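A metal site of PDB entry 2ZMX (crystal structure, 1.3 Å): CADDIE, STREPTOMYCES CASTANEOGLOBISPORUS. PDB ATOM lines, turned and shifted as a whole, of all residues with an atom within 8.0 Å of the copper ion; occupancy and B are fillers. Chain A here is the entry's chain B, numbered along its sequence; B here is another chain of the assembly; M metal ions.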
ATOM      1  N   HIS A  66       4.369  16.389  27.411  1.00  0.00           N
ATOM      2  CA  HIS A  66       3.250  16.273  26.485  1.00  0.00           C
ATOM      3  C   HIS A  66       2.690  17.649  26.113  1.00  0.00           C
ATOM      4  O   HIS A  66       1.741  17.723  25.332  1.00  0.00           O
ATOM      5  CB  HIS A  66       2.111  15.434  27.064  1.00  0.00           C
ATOM      6  CG  HIS A  66       2.245  13.955  26.834  1.00  0.00           C
ATOM      7  ND1 HIS A  66       2.786  13.420  25.689  1.00  0.00           N
ATOM      8  CD2 HIS A  66       1.895  12.915  27.616  1.00  0.00           C
ATOM      9  CE1 HIS A  66       2.764  12.105  25.779  1.00  0.00           C
ATOM     10  NE2 HIS A  66       2.225  11.770  26.937  1.00  0.00           N
ATOM     11  N   GLU A  67       3.285  18.687  26.686  1.00  0.00           N
ATOM     12  CA  GLU A  67       2.924  20.085  26.507  1.00  0.00           C
ATOM     13  C   GLU A  67       4.177  20.944  26.451  1.00  0.00           C
ATOM     14  O   GLU A  67       5.276  20.431  26.679  1.00  0.00           O
ATOM     15  CB  GLU A  67       2.011  20.581  27.638  1.00  0.00           C
ATOM     16  CG  GLU A  67       2.149  19.823  28.943  1.00  0.00           C
ATOM     17  CD  GLU A  67       3.042  20.486  29.974  1.00  0.00           C
ATOM     18  OE1 GLU A  67       3.653  21.544  29.691  1.00  0.00           O
ATOM     19  OE2 GLU A  67       3.160  19.955  31.095  1.00  0.00           O
ATOM     20  N   HIS A  68       4.000  22.228  26.172  1.00  0.00           N
ATOM     21  CA  HIS A  68       5.113  23.131  25.961  1.00  0.00           C
ATOM     22  C   HIS A  68       5.769  23.604  27.263  1.00  0.00           C
ATOM     23  O   HIS A  68       5.176  23.464  28.329  1.00  0.00           O
ATOM     24  CB  HIS A  68       4.637  24.380  25.212  1.00  0.00           C
ATOM     25  CG  HIS A  68       4.002  25.436  26.053  1.00  0.00           C
ATOM     26  ND1 HIS A  68       3.284  25.150  27.187  1.00  0.00           N
ATOM     27  CD2 HIS A  68       3.947  26.784  25.922  1.00  0.00           C
ATOM     28  CE1 HIS A  68       2.818  26.271  27.735  1.00  0.00           C
ATOM     29  NE2 HIS A  68       3.218  27.286  26.980  1.00  0.00           N
ATOM     30  N   GLY A  69       6.956  24.181  27.121  1.00  0.00           N
ATOM     31  CA  GLY A  69       7.769  24.798  28.156  1.00  0.00           C
ATOM     32  C   GLY A  69       6.984  25.381  29.312  1.00  0.00           C
ATOM     33  O   GLY A  69       6.563  24.640  30.217  1.00  0.00           O
ATOM     34  N   GLY A  70       6.774  26.699  29.332  1.00  0.00           N
ATOM     35  CA  GLY A  70       5.950  27.342  30.343  1.00  0.00           C
ATOM     36  C   GLY A  70       6.628  28.521  31.033  1.00  0.00           C
ATOM     37  O   GLY A  70       7.535  28.324  31.849  1.00  0.00           O
ATOM     38  N   GLY A  71       6.193  29.734  30.712  1.00  0.00           N
ATOM     39  CA  GLY A  71       6.686  30.941  31.328  1.00  0.00           C
ATOM     40  C   GLY A  71       5.689  31.459  32.365  1.00  0.00           C
ATOM     41  O   GLY A  71       6.000  32.388  33.108  1.00  0.00           O
ATOM     42  N   TYR A  72       4.489  30.883  32.380  1.00  0.00           N
ATOM     43  CA  TYR A  72       3.434  31.397  33.246  1.00  0.00           C
ATOM     44  C   TYR A  72       2.535  30.228  33.617  1.00  0.00           C
ATOM     45  O   TYR A  72       2.271  29.375  32.757  1.00  0.00           O
ATOM     46  CB  TYR A  72       2.654  32.516  32.539  1.00  0.00           C
ATOM     47  CG  TYR A  72       1.842  33.348  33.508  1.00  0.00           C
ATOM     48  CD1 TYR A  72       2.384  34.495  34.094  1.00  0.00           C
ATOM     49  CD2 TYR A  72       0.548  33.039  33.864  1.00  0.00           C
ATOM     50  CE1 TYR A  72       1.642  35.255  34.988  1.00  0.00           C
ATOM     51  CE2 TYR A  72      -0.176  33.794  34.750  1.00  0.00           C
ATOM     52  CZ  TYR A  72       0.357  34.944  35.341  1.00  0.00           C
ATOM     53  OH  TYR A  72      -0.412  35.652  36.210  1.00  0.00           O
ATOM     54  N   GLN A  80      -3.739  22.840  37.910  1.00  0.00           N
ATOM     55  CA  GLN A  80      -3.105  23.597  36.887  1.00  0.00           C
ATOM     56  C   GLN A  80      -3.865  23.566  35.550  1.00  0.00           C
ATOM     57  O   GLN A  80      -4.227  22.471  35.095  1.00  0.00           O
ATOM     58  CB  GLN A  80      -1.666  23.115  36.676  1.00  0.00           C
ATOM     59  CG  GLN A  80      -0.837  24.197  36.014  1.00  0.00           C
ATOM     60  CD  GLN A  80       0.620  23.914  35.789  1.00  0.00           C
ATOM     61  OE1 GLN A  80       1.169  24.579  34.912  1.00  0.00           O
ATOM     62  NE2 GLN A  80       1.176  23.010  36.567  1.00  0.00           N
ATOM     63  N   HIS A  82      -3.357  24.380  31.683  1.00  0.00           N
ATOM     64  CA  HIS A  82      -2.353  24.705  30.672  1.00  0.00           C
ATOM     65  C   HIS A  82      -2.766  25.912  29.866  1.00  0.00           C
ATOM     66  O   HIS A  82      -3.862  25.995  29.301  1.00  0.00           O
ATOM     67  CB  HIS A  82      -2.173  23.487  29.743  1.00  0.00           C
ATOM     68  CG  HIS A  82      -0.924  23.643  28.923  1.00  0.00           C
ATOM     69  ND1 HIS A  82      -0.943  24.123  27.655  1.00  0.00           N
ATOM     70  CD2 HIS A  82       0.381  23.371  29.220  1.00  0.00           C
ATOM     71  CE1 HIS A  82       0.292  24.162  27.168  1.00  0.00           C
ATOM     72  NE2 HIS A  82       1.107  23.696  28.103  1.00  0.00           N
ATOM     73  N   VAL A  83      -1.853  26.882  29.794  1.00  0.00           N
ATOM     74  CA  VAL A  83      -2.080  28.112  29.053  1.00  0.00           C
ATOM     75  C   VAL A  83      -0.866  28.373  28.190  1.00  0.00           C
ATOM     76  O   VAL A  83       0.250  27.897  28.431  1.00  0.00           O
ATOM     77  CB  VAL A  83      -2.381  29.334  29.966  1.00  0.00           C
ATOM     78  CG1 VAL A  83      -3.663  29.113  30.757  1.00  0.00           C
ATOM     79  CG2 VAL A  83      -1.238  29.681  30.900  1.00  0.00           C
ATOM     80  N   MET A  84      -1.118  29.171  27.154  1.00  0.00           N
ATOM     81  CA  MET A  84      -0.029  29.432  26.216  1.00  0.00           C
ATOM     82  C   MET A  84      -0.123  30.844  25.695  1.00  0.00           C
ATOM     83  O   MET A  84      -1.202  31.379  25.470  1.00  0.00           O
ATOM     84  CB  MET A  84      -0.071  28.390  25.117  1.00  0.00           C
ATOM     85  CG  MET A  84       0.130  28.825  23.690  1.00  0.00           C
ATOM     86  SD  MET A  84       0.329  27.408  22.583  1.00  0.00           S
ATOM     87  CE  MET A  84      -0.148  26.047  23.683  1.00  0.00           C
ATOM     88  N   ILE B  42      -1.203  20.143  19.868  1.00  0.00           N
ATOM     89  CA  ILE B  42      -1.665  21.511  20.027  1.00  0.00           C
ATOM     90  C   ILE B  42      -1.162  22.138  21.322  1.00  0.00           C
ATOM     91  O   ILE B  42      -0.938  23.348  21.411  1.00  0.00           O
ATOM     92  CB  ILE B  42      -3.190  21.478  19.913  1.00  0.00           C
ATOM     93  CG1 ILE B  42      -3.715  22.795  19.312  1.00  0.00           C
ATOM     94  CG2 ILE B  42      -3.816  21.115  21.242  1.00  0.00           C
ATOM     95  CD1 ILE B  42      -5.096  22.599  18.727  1.00  0.00           C
ATOM     96  N   MET B  43      -0.890  21.320  22.317  1.00  0.00           N
ATOM     97  CA  MET B  43      -0.340  21.816  23.573  1.00  0.00           C
ATOM     98  C   MET B  43       1.162  22.041  23.518  1.00  0.00           C
ATOM     99  O   MET B  43       1.674  22.712  24.414  1.00  0.00           O
ATOM    100  CB  MET B  43      -0.614  20.815  24.687  1.00  0.00           C
ATOM    101  CG  MET B  43      -2.083  20.711  25.054  1.00  0.00           C
ATOM    102  SD  MET B  43      -2.290  19.658  26.490  1.00  0.00           S
ATOM    103  CE  MET B  43      -2.225  20.816  27.836  1.00  0.00           C
ATOM    104  N   SER B  44       1.854  21.479  22.517  1.00  0.00           N
ATOM    105  CA  SER B  44       3.302  21.710  22.441  1.00  0.00           C
ATOM    106  C   SER B  44       3.745  22.689  21.360  1.00  0.00           C
ATOM    107  O   SER B  44       4.800  23.352  21.493  1.00  0.00           O
ATOM    108  CB  SER B  44       4.000  20.366  22.209  1.00  0.00           C
ATOM    109  OG  SER B  44       3.627  19.742  20.996  1.00  0.00           O
ATOM    110  N   ASP B  45       3.002  22.804  20.261  1.00  0.00           N
ATOM    111  CA  ASP B  45       3.348  23.750  19.212  1.00  0.00           C
ATOM    112  C   ASP B  45       3.402  25.174  19.757  1.00  0.00           C
ATOM    113  O   ASP B  45       2.382  25.578  20.327  1.00  0.00           O
ATOM    114  CB  ASP B  45       2.350  23.676  18.054  1.00  0.00           C
ATOM    115  CG  ASP B  45       2.346  22.409  17.226  1.00  0.00           C
ATOM    116  OD1 ASP B  45       1.247  22.114  16.648  1.00  0.00           O
ATOM    117  OD2 ASP B  45       3.379  21.710  17.113  1.00  0.00           O
ATOM    118  N   THR B  46       4.493  25.932  19.662  1.00  0.00           N
ATOM    119  CA  THR B  46       4.477  27.273  20.279  1.00  0.00           C
ATOM    120  C   THR B  46       5.072  28.252  19.280  1.00  0.00           C
ATOM    121  O   THR B  46       5.901  27.866  18.460  1.00  0.00           O
ATOM    122  CB  THR B  46       5.270  27.370  21.597  1.00  0.00           C
ATOM    123  OG1 THR B  46       6.638  26.950  21.415  1.00  0.00           O
ATOM    124  CG2 THR B  46       4.693  26.455  22.645  1.00  0.00           C
HETATM  125 CU    CU M   1       3.131  23.539  28.183  1.00  0.00          CU
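Three residues have an atom within 4 Å of the copper ion: Glu 67, His 68 and His 82. The nearest printed residue that does not touch the copper ion is Gly 69 (4.02 Å).
The backbone carbonyl oxygen of Val 83 lies close to a ring nitrogen (NE2) of His 68 (3.4 Å). N of His 68 sits close to O of Met 43 of chain B, 3.0 Å away.
The copper ion is bound by ND1 of His 68 (1.9 Å), NE2 of His 82 (2.0 Å), O of His 68 (2.1 Å), N of His 68 (2.6 Å) and OE1 of Glu 67 (2.6 Å).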
